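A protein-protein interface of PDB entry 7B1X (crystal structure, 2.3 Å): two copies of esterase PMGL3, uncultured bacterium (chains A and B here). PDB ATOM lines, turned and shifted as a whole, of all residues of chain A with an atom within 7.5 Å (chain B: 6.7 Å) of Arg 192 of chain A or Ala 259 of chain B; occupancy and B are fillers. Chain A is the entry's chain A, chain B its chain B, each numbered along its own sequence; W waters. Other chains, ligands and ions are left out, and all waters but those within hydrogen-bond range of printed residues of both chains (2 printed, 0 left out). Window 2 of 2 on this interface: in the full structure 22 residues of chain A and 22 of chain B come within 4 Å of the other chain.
No position is printed for both chains.
Of the 11 pairs that touch across the chains among the printed residues, none has its exchanged pair printed and touching as well.
The guanidinium group (NH1) of Arg 192 of chain A lies within hydrogen-bond range of the backbone carbonyl oxygen (O) of Leu 258 of chain B (2.9 Å).
Water W2 bridges OG of Ser 247 of chain A and NE of Arg 254 of chain B.
Water W1 lies within hydrogen-bond range of OD1 of Asp 242 of chain A (2.6 Å), N of Asn 270 of chain A (2.9 Å) and O of Gly 260 of chain B (3.0 Å).
The backbone NH (N) of Ala 187 of chain A sits at hydrogen-bond distance from the side-chain hydroxyl (OG) of Ser 247 of chain A, at 3.4 Å.
The backbone NH (N) of Gly 193 of chain A lies within hydrogen-bond range of the backbone carbonyl oxygen (O) of Ser 188 of chain A (3.3 Å).
The backbone carbonyl oxygen of Val 244 of chain A lies within hydrogen-bond range of the side-chain hydroxyl of Ser 188 of chain A (2.5 Å).
The side-chain hydroxyl of Ser 188 of chain A sits at hydrogen-bond distance from the backbone NH of Ser 247 of chain A (2.8 Å).
O of Ala 241 of chain A sits at hydrogen-bond distance from NE of Arg 192 of chain A (2.8 Å).
The guanidinium group (NH2) of Arg 192 of chain A lies within salt-bridge range of the side-chain carboxylate (OD1) of Asp 242 of chain A.
Arg 192 of chain A touches just these residues of chain B: Ala 257, Leu 258, Ala 259 and Gly 260.
Ala 259 of chain B touches just one residue of chain A: Arg 192 (3.9 Å).
Printed residues of chain B within 4 Å of Ala 269 of chain A: Gly 260.
Printed residues of chain A within 4 Å of Arg 254 of chain B: Ala 187.
Of the printed residues of chain B, Ser 188 of chain A touches Leu 258 (3.9 Å).
Val 244 of chain A touches none of the printed residues of chain B.
Asp 242 of chain A touches none of the printed residues of chain B.
The nearest residue of chain B that does not touch Arg 192 of chain A is Leu 261 of chain B (6.1 Å).
The nearest printed residue of chain B that does not touch Leu 246 of chain A is Arg 254 of chain B (5.4 Å).
Of the 14 printed residues of chain B, 5 touch a printed residue of chain A.
Hydrophobic or aromatic side chains of chain B that line the printed part of chain A: Ala 257 and Leu 258.
Among the printed residues, no Asp or Glu carboxylate lies within 4 Å of a Lys or Arg side-chain nitrogen of the other chain.
Among the printed residues, pairs that only touch across the chains: Ala 187 of chain A with Arg 254 of chain B, Ala 187 of chain A with Leu 258 of chain B, Ser 188 of chain A with Leu 258 of chain B, Arg 192 of chain A with Ala 257 of chain B, Arg 192 of chain A with Ala 259 of chain B, Arg 192 of chain A with Gly 260 of chain B, Ala 241 of chain A with Gly 260 of chain B, Leu 246 of chain A with Ala 257 of chain B, Leu 246 of chain A with Leu 258 of chain B and Ala 269 of chain A with Gly 260 of chain B.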
ATOM      1  N   LYS A  12     -21.487  16.018 -34.028  1.00  0.00           N
ATOM      2  CA  LYS A  12     -21.384  17.350 -33.461  1.00  0.00           C
ATOM      3  C   LYS A  12     -21.409  18.415 -34.555  1.00  0.00           C
ATOM      4  O   LYS A  12     -22.125  19.402 -34.366  1.00  0.00           O
ATOM      5  CB  LYS A  12     -20.194  17.472 -32.488  1.00  0.00           C
ATOM      6  CG  LYS A  12     -20.422  16.875 -31.090  1.00  0.00           C
ATOM      7  CD  LYS A  12     -19.190  16.938 -30.203  1.00  0.00           C
ATOM      8  CE  LYS A  12     -19.474  16.980 -28.714  1.00  0.00           C
ATOM      9  NZ  LYS A  12     -18.194  16.935 -27.948  1.00  0.00           N
ATOM     10  N   GLY A 186     -27.587  28.337 -14.439  1.00  0.00           N
ATOM     11  CA  GLY A 186     -26.561  27.411 -14.017  1.00  0.00           C
ATOM     12  C   GLY A 186     -25.246  27.764 -14.676  1.00  0.00           C
ATOM     13  O   GLY A 186     -25.246  28.252 -15.801  1.00  0.00           O
ATOM     14  N   ALA A 187     -24.150  27.452 -13.990  1.00  0.00           N
ATOM     15  CA  ALA A 187     -22.792  27.640 -14.473  1.00  0.00           C
ATOM     16  C   ALA A 187     -22.633  27.087 -15.880  1.00  0.00           C
ATOM     17  O   ALA A 187     -21.860  27.639 -16.661  1.00  0.00           O
ATOM     18  CB  ALA A 187     -21.831  26.971 -13.520  1.00  0.00           C
ATOM     19  N   SER A 188     -23.399  26.023 -16.223  1.00  0.00           N
ATOM     20  CA  SER A 188     -23.162  25.254 -17.440  1.00  0.00           C
ATOM     21  C   SER A 188     -23.557  26.005 -18.729  1.00  0.00           C
ATOM     22  O   SER A 188     -22.942  25.760 -19.769  1.00  0.00           O
ATOM     23  CB  SER A 188     -23.810  23.880 -17.359  1.00  0.00           C
ATOM     24  OG  SER A 188     -25.248  23.939 -17.212  1.00  0.00           O
ATOM     25  N   TYR A 189     -24.580  26.891 -18.680  1.00  0.00           N
ATOM     26  CA  TYR A 189     -24.908  27.805 -19.791  1.00  0.00           C
ATOM     27  C   TYR A 189     -23.666  28.490 -20.348  1.00  0.00           C
ATOM     28  O   TYR A 189     -23.409  28.440 -21.552  1.00  0.00           O
ATOM     29  CB  TYR A 189     -25.995  28.849 -19.452  1.00  0.00           C
ATOM     30  CG  TYR A 189     -27.331  28.165 -19.341  1.00  0.00           C
ATOM     31  CD1 TYR A 189     -28.057  27.835 -20.488  1.00  0.00           C
ATOM     32  CD2 TYR A 189     -27.751  27.657 -18.101  1.00  0.00           C
ATOM     33  CE1 TYR A 189     -29.237  27.101 -20.390  1.00  0.00           C
ATOM     34  CE2 TYR A 189     -28.928  26.926 -17.987  1.00  0.00           C
ATOM     35  CZ  TYR A 189     -29.658  26.630 -19.138  1.00  0.00           C
ATOM     36  OH  TYR A 189     -30.825  25.928 -19.028  1.00  0.00           O
ATOM     37  N   GLU A 190     -22.874  29.058 -19.439  1.00  0.00           N
ATOM     38  CA  GLU A 190     -21.677  29.775 -19.834  1.00  0.00           C
ATOM     39  C   GLU A 190     -20.577  28.746 -20.084  1.00  0.00           C
ATOM     40  O   GLU A 190     -19.892  28.850 -21.099  1.00  0.00           O
ATOM     41  CB  GLU A 190     -21.280  30.790 -18.755  1.00  0.00           C
ATOM     42  CG  GLU A 190     -20.685  32.082 -19.277  1.00  0.00           C
ATOM     43  CD  GLU A 190     -19.295  32.491 -18.763  1.00  0.00           C
ATOM     44  OE1 GLU A 190     -19.116  32.668 -17.526  1.00  0.00           O
ATOM     45  OE2 GLU A 190     -18.368  32.653 -19.620  1.00  0.00           O
ATOM     46  N   ALA A 191     -20.392  27.824 -19.119  1.00  0.00           N
ATOM     47  CA  ALA A 191     -19.225  26.958 -19.091  1.00  0.00           C
ATOM     48  C   ALA A 191     -19.340  25.910 -20.202  1.00  0.00           C
ATOM     49  O   ALA A 191     -18.335  25.601 -20.856  1.00  0.00           O
ATOM     50  CB  ALA A 191     -18.989  26.376 -17.704  1.00  0.00           C
ATOM     51  N   ARG A 192     -20.561  25.416 -20.478  1.00  0.00           N
ATOM     52  CA  ARG A 192     -20.679  24.313 -21.438  1.00  0.00           C
ATOM     53  C   ARG A 192     -21.202  24.777 -22.784  1.00  0.00           C
ATOM     54  O   ARG A 192     -21.033  24.064 -23.773  1.00  0.00           O
ATOM     55  CB  ARG A 192     -21.400  23.072 -20.867  1.00  0.00           C
ATOM     56  CG  ARG A 192     -20.907  22.613 -19.497  1.00  0.00           C
ATOM     57  CD  ARG A 192     -19.416  22.499 -19.272  1.00  0.00           C
ATOM     58  NE  ARG A 192     -19.031  21.577 -20.310  1.00  0.00           N
ATOM     59  CZ  ARG A 192     -17.831  21.381 -20.832  1.00  0.00           C
ATOM     60  NH1 ARG A 192     -16.782  22.059 -20.401  1.00  0.00           N
ATOM     61  NH2 ARG A 192     -17.705  20.499 -21.806  1.00  0.00           N
ATOM     62  N   GLY A 193     -21.757  26.002 -22.819  1.00  0.00           N
ATOM     63  CA  GLY A 193     -22.440  26.609 -23.964  1.00  0.00           C
ATOM     64  C   GLY A 193     -21.618  26.520 -25.241  1.00  0.00           C
ATOM     65  O   GLY A 193     -22.124  26.073 -26.248  1.00  0.00           O
ATOM     66  N   PRO A 194     -20.317  26.904 -25.249  1.00  0.00           N
ATOM     67  CA  PRO A 194     -19.473  26.703 -26.434  1.00  0.00           C
ATOM     68  C   PRO A 194     -19.306  25.239 -26.833  1.00  0.00           C
ATOM     69  O   PRO A 194     -18.859  24.974 -27.945  1.00  0.00           O
ATOM     70  CB  PRO A 194     -18.100  27.229 -26.004  1.00  0.00           C
ATOM     71  CG  PRO A 194     -18.412  28.249 -24.901  1.00  0.00           C
ATOM     72  CD  PRO A 194     -19.623  27.660 -24.188  1.00  0.00           C
ATOM     73  N   HIS A 195     -19.627  24.272 -25.941  1.00  0.00           N
ATOM     74  CA  HIS A 195     -19.416  22.865 -26.265  1.00  0.00           C
ATOM     75  C   HIS A 195     -20.732  22.183 -26.605  1.00  0.00           C
ATOM     76  O   HIS A 195     -20.696  21.024 -27.049  1.00  0.00           O
ATOM     77  CB  HIS A 195     -18.714  22.134 -25.139  1.00  0.00           C
ATOM     78  CG  HIS A 195     -17.436  22.797 -24.766  1.00  0.00           C
ATOM     79  ND1 HIS A 195     -16.284  22.676 -25.540  1.00  0.00           N
ATOM     80  CD2 HIS A 195     -17.120  23.622 -23.749  1.00  0.00           C
ATOM     81  CE1 HIS A 195     -15.308  23.337 -24.978  1.00  0.00           C
ATOM     82  NE2 HIS A 195     -15.799  23.905 -23.886  1.00  0.00           N
ATOM     83  N   ASP A 196     -21.852  22.903 -26.388  1.00  0.00           N
ATOM     84  CA  ASP A 196     -23.178  22.331 -26.590  1.00  0.00           C
ATOM     85  C   ASP A 196     -23.619  22.713 -27.984  1.00  0.00           C
ATOM     86  O   ASP A 196     -24.083  23.831 -28.172  1.00  0.00           O
ATOM     87  CB  ASP A 196     -24.228  22.728 -25.536  1.00  0.00           C
ATOM     88  CG  ASP A 196     -25.595  22.013 -25.666  1.00  0.00           C
ATOM     89  OD1 ASP A 196     -25.948  21.578 -26.823  1.00  0.00           O
ATOM     90  OD2 ASP A 196     -26.333  21.887 -24.609  1.00  0.00           O
ATOM     91  N   PRO A 197     -23.545  21.803 -28.985  1.00  0.00           N
ATOM     92  CA  PRO A 197     -23.973  22.157 -30.346  1.00  0.00           C
ATOM     93  C   PRO A 197     -25.470  22.021 -30.577  1.00  0.00           C
ATOM     94  O   PRO A 197     -25.943  22.310 -31.661  1.00  0.00           O
ATOM     95  CB  PRO A 197     -23.180  21.184 -31.214  1.00  0.00           C
ATOM     96  CG  PRO A 197     -23.047  19.934 -30.344  1.00  0.00           C
ATOM     97  CD  PRO A 197     -23.016  20.424 -28.898  1.00  0.00           C
ATOM     98  N   ILE A 199     -28.315  22.455 -27.963  1.00  0.00           N
ATOM     99  CA  ILE A 199     -29.233  23.156 -27.084  1.00  0.00           C
ATOM    100  C   ILE A 199     -28.649  24.533 -26.745  1.00  0.00           C
ATOM    101  O   ILE A 199     -27.525  24.631 -26.226  1.00  0.00           O
ATOM    102  CB  ILE A 199     -29.488  22.305 -25.821  1.00  0.00           C
ATOM    103  CG1 ILE A 199     -30.074  20.954 -26.211  1.00  0.00           C
ATOM    104  CG2 ILE A 199     -30.396  23.028 -24.852  1.00  0.00           C
ATOM    105  CD1 ILE A 199     -31.465  21.103 -26.830  1.00  0.00           C
ATOM    106  N   GLY A 240     -24.895  14.588 -20.503  1.00  0.00           N
ATOM    107  CA  GLY A 240     -23.607  14.738 -21.154  1.00  0.00           C
ATOM    108  C   GLY A 240     -22.892  15.948 -20.574  1.00  0.00           C
ATOM    109  O   GLY A 240     -23.544  16.869 -20.061  1.00  0.00           O
ATOM    110  N   ALA A 241     -21.547  15.945 -20.645  1.00  0.00           N
ATOM    111  CA  ALA A 241     -20.699  17.012 -20.147  1.00  0.00           C
ATOM    112  C   ALA A 241     -20.851  18.214 -21.068  1.00  0.00           C
ATOM    113  O   ALA A 241     -20.703  19.358 -20.597  1.00  0.00           O
ATOM    114  CB  ALA A 241     -19.254  16.597 -20.046  1.00  0.00           C
ATOM    115  N   ASP A 242     -21.219  17.943 -22.342  1.00  0.00           N
ATOM    116  CA  ASP A 242     -21.244  19.006 -23.341  1.00  0.00           C
ATOM    117  C   ASP A 242     -22.655  19.556 -23.514  1.00  0.00           C
ATOM    118  O   ASP A 242     -23.197  19.532 -24.621  1.00  0.00           O
ATOM    119  CB  ASP A 242     -20.631  18.509 -24.653  1.00  0.00           C
ATOM    120  CG  ASP A 242     -19.155  18.221 -24.508  1.00  0.00           C
ATOM    121  OD1 ASP A 242     -18.584  18.532 -23.424  1.00  0.00           O
ATOM    122  OD2 ASP A 242     -18.582  17.702 -25.476  1.00  0.00           O
ATOM    123  N   GLU A 243     -23.263  19.986 -22.395  1.00  0.00           N
ATOM    124  CA  GLU A 243     -24.676  20.317 -22.320  1.00  0.00           C
ATOM    125  C   GLU A 243     -24.893  21.582 -21.479  1.00  0.00           C
ATOM    126  O   GLU A 243     -24.477  21.621 -20.307  1.00  0.00           O
ATOM    127  CB  GLU A 243     -25.389  19.204 -21.578  1.00  0.00           C
ATOM    128  CG  GLU A 243     -25.690  18.012 -22.447  1.00  0.00           C
ATOM    129  CD  GLU A 243     -27.029  17.364 -22.052  1.00  0.00           C
ATOM    130  OE1 GLU A 243     -28.069  17.994 -22.189  1.00  0.00           O
ATOM    131  OE2 GLU A 243     -27.034  16.192 -21.616  1.00  0.00           O
ATOM    132  N   VAL A 244     -25.605  22.582 -22.037  1.00  0.00           N
ATOM    133  CA  VAL A 244     -26.032  23.719 -21.234  1.00  0.00           C
ATOM    134  C   VAL A 244     -26.917  23.271 -20.059  1.00  0.00           C
ATOM    135  O   VAL A 244     -26.961  23.927 -19.006  1.00  0.00           O
ATOM    136  CB  VAL A 244     -26.708  24.821 -22.078  1.00  0.00           C
ATOM    137  CG1 VAL A 244     -25.758  25.504 -23.060  1.00  0.00           C
ATOM    138  CG2 VAL A 244     -27.948  24.306 -22.798  1.00  0.00           C
ATOM    139  N   LEU A 245     -27.644  22.184 -20.220  1.00  0.00           N
ATOM    140  CA  LEU A 245     -28.527  21.644 -19.193  1.00  0.00           C
ATOM    141  C   LEU A 245     -27.801  20.825 -18.107  1.00  0.00           C
ATOM    142  O   LEU A 245     -28.481  20.394 -17.177  1.00  0.00           O
ATOM    143  CB  LEU A 245     -29.590  20.775 -19.864  1.00  0.00           C
ATOM    144  CG  LEU A 245     -30.737  21.549 -20.516  1.00  0.00           C
ATOM    145  CD1 LEU A 245     -31.604  20.564 -21.259  1.00  0.00           C
ATOM    146  CD2 LEU A 245     -31.533  22.359 -19.464  1.00  0.00           C
ATOM    147  N   LEU A 246     -26.441  20.684 -18.191  1.00  0.00           N
ATOM    148  CA  LEU A 246     -25.588  19.977 -17.230  1.00  0.00           C
ATOM    149  C   LEU A 246     -25.892  20.397 -15.776  1.00  0.00           C
ATOM    150  O   LEU A 246     -26.135  19.538 -14.910  1.00  0.00           O
ATOM    151  CB  LEU A 246     -24.089  20.160 -17.570  1.00  0.00           C
ATOM    152  CG  LEU A 246     -23.137  19.495 -16.593  1.00  0.00           C
ATOM    153  CD1 LEU A 246     -23.322  17.945 -16.561  1.00  0.00           C
ATOM    154  CD2 LEU A 246     -21.708  19.912 -16.890  1.00  0.00           C
ATOM    155  N   SER A 247     -25.865  21.722 -15.535  1.00  0.00           N
ATOM    156  CA  SER A 247     -26.093  22.288 -14.213  1.00  0.00           C
ATOM    157  C   SER A 247     -27.413  21.798 -13.587  1.00  0.00           C
ATOM    158  O   SER A 247     -27.401  21.588 -12.382  1.00  0.00           O
ATOM    159  CB  SER A 247     -25.956  23.806 -14.177  1.00  0.00           C
ATOM    160  OG  SER A 247     -24.582  24.129 -14.211  1.00  0.00           O
ATOM    161  N   ALA A 269     -18.325  12.208 -20.674  1.00  0.00           N
ATOM    162  CA  ALA A 269     -17.459  13.124 -21.395  1.00  0.00           C
ATOM    163  C   ALA A 269     -17.866  13.113 -22.870  1.00  0.00           C
ATOM    164  O   ALA A 269     -18.327  12.069 -23.374  1.00  0.00           O
ATOM    165  CB  ALA A 269     -15.985  12.817 -21.189  1.00  0.00           C
ATOM    166  N   ASN A 270     -17.757  14.289 -23.502  1.00  0.00           N
ATOM    167  CA  ASN A 270     -17.977  14.456 -24.934  1.00  0.00           C
ATOM    168  C   ASN A 270     -19.395  14.283 -25.450  1.00  0.00           C
ATOM    169  O   ASN A 270     -19.618  14.491 -26.645  1.00  0.00           O
ATOM    170  CB  ASN A 270     -17.300  13.398 -25.774  1.00  0.00           C
ATOM    171  CG  ASN A 270     -15.936  13.940 -26.024  1.00  0.00           C
ATOM    172  OD1 ASN A 270     -15.056  13.652 -25.222  1.00  0.00           O
ATOM    173  ND2 ASN A 270     -15.836  14.845 -26.995  1.00  0.00           N
ATOM    174  N   MET A 271     -20.338  14.007 -24.562  1.00  0.00           N
ATOM    175  CA  MET A 271     -21.669  13.637 -25.044  1.00  0.00           C
ATOM    176  C   MET A 271     -22.553  14.873 -25.106  1.00  0.00           C
ATOM    177  O   MET A 271     -22.558  15.742 -24.199  1.00  0.00           O
ATOM    178  CB  MET A 271     -22.351  12.536 -24.196  1.00  0.00           C
ATOM    179  CG  MET A 271     -21.843  11.123 -24.482  1.00  0.00           C
ATOM    180  SD  MET A 271     -21.891  10.783 -26.208  1.00  0.00           S
ATOM    181  CE  MET A 271     -20.146  10.852 -26.628  1.00  0.00           C
ATOM    182  N   ASP B 228      -9.980  24.411 -10.199  1.00  0.00           N
ATOM    183  CA  ASP B 228     -10.479  24.275 -11.544  1.00  0.00           C
ATOM    184  C   ASP B 228      -9.989  22.902 -12.004  1.00  0.00           C
ATOM    185  O   ASP B 228      -8.825  22.547 -11.828  1.00  0.00           O
ATOM    186  CB  ASP B 228     -10.262  25.574 -12.319  1.00  0.00           C
ATOM    187  CG  ASP B 228     -10.299  25.486 -13.846  1.00  0.00           C
ATOM    188  OD1 ASP B 228     -10.807  24.474 -14.425  1.00  0.00           O
ATOM    189  OD2 ASP B 228      -9.816  26.469 -14.493  1.00  0.00           O
ATOM    190  N   LEU B 229     -10.915  22.112 -12.542  1.00  0.00           N
ATOM    191  CA  LEU B 229     -10.604  20.697 -12.730  1.00  0.00           C
ATOM    192  C   LEU B 229     -10.240  20.353 -14.187  1.00  0.00           C
ATOM    193  O   LEU B 229     -10.202  19.167 -14.551  1.00  0.00           O
ATOM    194  CB  LEU B 229     -11.725  19.793 -12.165  1.00  0.00           C
ATOM    195  CG  LEU B 229     -12.064  19.933 -10.683  1.00  0.00           C
ATOM    196  CD1 LEU B 229     -12.909  18.750 -10.212  1.00  0.00           C
ATOM    197  CD2 LEU B 229     -10.808  19.944  -9.845  1.00  0.00           C
ATOM    198  N   ALA B 230      -9.937  21.367 -15.015  1.00  0.00           N
ATOM    199  CA  ALA B 230      -9.604  21.206 -16.432  1.00  0.00           C
ATOM    200  C   ALA B 230      -8.541  20.126 -16.582  1.00  0.00           C
ATOM    201  O   ALA B 230      -7.573  20.148 -15.834  1.00  0.00           O
ATOM    202  CB  ALA B 230      -9.143  22.525 -17.026  1.00  0.00           C
ATOM    203  N   ASP B 231      -8.791  19.124 -17.447  1.00  0.00           N
ATOM    204  CA  ASP B 231      -7.772  18.168 -17.887  1.00  0.00           C
ATOM    205  C   ASP B 231      -7.512  17.039 -16.885  1.00  0.00           C
ATOM    206  O   ASP B 231      -6.655  16.182 -17.161  1.00  0.00           O
ATOM    207  CB  ASP B 231      -6.501  18.884 -18.381  1.00  0.00           C
ATOM    208  CG  ASP B 231      -6.800  19.742 -19.614  1.00  0.00           C
ATOM    209  OD1 ASP B 231      -7.220  19.156 -20.638  1.00  0.00           O
ATOM    210  OD2 ASP B 231      -6.681  20.987 -19.535  1.00  0.00           O
ATOM    211  N   LEU B 232      -8.253  16.999 -15.750  1.00  0.00           N
ATOM    212  CA  LEU B 232      -8.136  15.835 -14.879  1.00  0.00           C
ATOM    213  C   LEU B 232      -8.725  14.621 -15.599  1.00  0.00           C
ATOM    214  O   LEU B 232      -9.447  14.798 -16.608  1.00  0.00           O
ATOM    215  CB  LEU B 232      -8.785  16.039 -13.500  1.00  0.00           C
ATOM    216  CG  LEU B 232      -8.190  17.078 -12.546  1.00  0.00           C
ATOM    217  CD1 LEU B 232      -8.398  16.705 -11.083  1.00  0.00           C
ATOM    218  CD2 LEU B 232      -6.739  17.453 -12.837  1.00  0.00           C
ATOM    219  N   THR B 253     -17.852  16.885  -8.065  1.00  0.00           N
ATOM    220  CA  THR B 253     -18.615  16.400  -9.207  1.00  0.00           C
ATOM    221  C   THR B 253     -19.012  17.568 -10.108  1.00  0.00           C
ATOM    222  O   THR B 253     -18.727  17.583 -11.298  1.00  0.00           O
ATOM    223  CB  THR B 253     -19.820  15.570  -8.747  1.00  0.00           C
ATOM    224  OG1 THR B 253     -19.253  14.500  -7.996  1.00  0.00           O
ATOM    225  CG2 THR B 253     -20.507  14.956  -9.942  1.00  0.00           C
ATOM    226  N   ARG B 254     -19.641  18.568  -9.520  1.00  0.00           N
ATOM    227  CA  ARG B 254     -20.040  19.772 -10.249  1.00  0.00           C
ATOM    228  C   ARG B 254     -18.857  20.317 -11.061  1.00  0.00           C
ATOM    229  O   ARG B 254     -18.967  20.554 -12.251  1.00  0.00           O
ATOM    230  CB  ARG B 254     -20.574  20.784  -9.230  1.00  0.00           C
ATOM    231  CG  ARG B 254     -21.466  21.889  -9.784  1.00  0.00           C
ATOM    232  CD  ARG B 254     -21.784  22.782  -8.601  1.00  0.00           C
ATOM    233  NE  ARG B 254     -21.536  23.965  -9.341  1.00  0.00           N
ATOM    234  CZ  ARG B 254     -20.532  24.817  -9.272  1.00  0.00           C
ATOM    235  NH1 ARG B 254     -19.614  24.800  -8.315  1.00  0.00           N
ATOM    236  NH2 ARG B 254     -20.567  25.743 -10.199  1.00  0.00           N
ATOM    237  N   ARG B 255     -17.697  20.450 -10.405  1.00  0.00           N
ATOM    238  CA  ARG B 255     -16.541  21.082 -11.013  1.00  0.00           C
ATOM    239  C   ARG B 255     -15.975  20.230 -12.132  1.00  0.00           C
ATOM    240  O   ARG B 255     -15.558  20.807 -13.133  1.00  0.00           O
ATOM    241  CB  ARG B 255     -15.517  21.534  -9.965  1.00  0.00           C
ATOM    242  CG  ARG B 255     -15.973  22.839  -9.324  1.00  0.00           C
ATOM    243  CD  ARG B 255     -15.183  23.002  -8.050  1.00  0.00           C
ATOM    244  NE  ARG B 255     -15.488  24.271  -7.421  1.00  0.00           N
ATOM    245  CZ  ARG B 255     -14.749  25.370  -7.372  1.00  0.00           C
ATOM    246  NH1 ARG B 255     -13.546  25.483  -7.908  1.00  0.00           N
ATOM    247  NH2 ARG B 255     -15.242  26.412  -6.745  1.00  0.00           N
ATOM    248  N   ALA B 256     -15.929  18.901 -11.902  1.00  0.00           N
ATOM    249  CA  ALA B 256     -15.473  17.920 -12.865  1.00  0.00           C
ATOM    250  C   ALA B 256     -16.339  18.013 -14.104  1.00  0.00           C
ATOM    251  O   ALA B 256     -15.817  18.173 -15.209  1.00  0.00           O
ATOM    252  CB  ALA B 256     -15.457  16.519 -12.280  1.00  0.00           C
ATOM    253  N   ALA B 257     -17.658  18.046 -13.886  1.00  0.00           N
ATOM    254  CA  ALA B 257     -18.623  18.117 -14.975  1.00  0.00           C
ATOM    255  C   ALA B 257     -18.408  19.401 -15.771  1.00  0.00           C
ATOM    256  O   ALA B 257     -18.396  19.416 -16.997  1.00  0.00           O
ATOM    257  CB  ALA B 257     -20.026  18.046 -14.392  1.00  0.00           C
ATOM    258  N   LEU B 258     -18.207  20.496 -15.051  1.00  0.00           N
ATOM    259  CA  LEU B 258     -18.101  21.808 -15.675  1.00  0.00           C
ATOM    260  C   LEU B 258     -16.804  21.906 -16.491  1.00  0.00           C
ATOM    261  O   LEU B 258     -16.751  22.581 -17.524  1.00  0.00           O
ATOM    262  CB  LEU B 258     -18.160  22.825 -14.534  1.00  0.00           C
ATOM    263  CG  LEU B 258     -19.421  23.670 -14.327  1.00  0.00           C
ATOM    264  CD1 LEU B 258     -20.623  23.288 -15.167  1.00  0.00           C
ATOM    265  CD2 LEU B 258     -19.766  23.760 -12.866  1.00  0.00           C
ATOM    266  N   ALA B 259     -15.755  21.204 -16.040  1.00  0.00           N
ATOM    267  CA  ALA B 259     -14.507  21.076 -16.792  1.00  0.00           C
ATOM    268  C   ALA B 259     -14.646  20.041 -17.910  1.00  0.00           C
ATOM    269  O   ALA B 259     -13.689  19.809 -18.644  1.00  0.00           O
ATOM    270  CB  ALA B 259     -13.343  20.717 -15.884  1.00  0.00           C
ATOM    271  N   GLY B 260     -15.804  19.380 -18.020  1.00  0.00           N
ATOM    272  CA  GLY B 260     -16.042  18.492 -19.161  1.00  0.00           C
ATOM    273  C   GLY B 260     -15.622  17.033 -18.930  1.00  0.00           C
ATOM    274  O   GLY B 260     -15.693  16.231 -19.844  1.00  0.00           O
ATOM    275  N   LEU B 261     -15.252  16.675 -17.703  1.00  0.00           N
ATOM    276  CA  LEU B 261     -14.748  15.358 -17.335  1.00  0.00           C
ATOM    277  C   LEU B 261     -15.884  14.335 -17.310  1.00  0.00           C
ATOM    278  O   LEU B 261     -17.050  14.649 -17.020  1.00  0.00           O
ATOM    279  CB  LEU B 261     -14.090  15.449 -15.943  1.00  0.00           C
ATOM    280  CG  LEU B 261     -12.644  15.958 -15.810  1.00  0.00           C
ATOM    281  CD1 LEU B 261     -12.224  16.972 -16.868  1.00  0.00           C
ATOM    282  CD2 LEU B 261     -12.359  16.492 -14.432  1.00  0.00           C
HETATM  283  O   HOH W   1     -16.735  16.834 -22.581  1.00  0.00           O
HETATM  284  O   HOH W   2     -23.380  24.177 -12.077  1.00  0.00           O
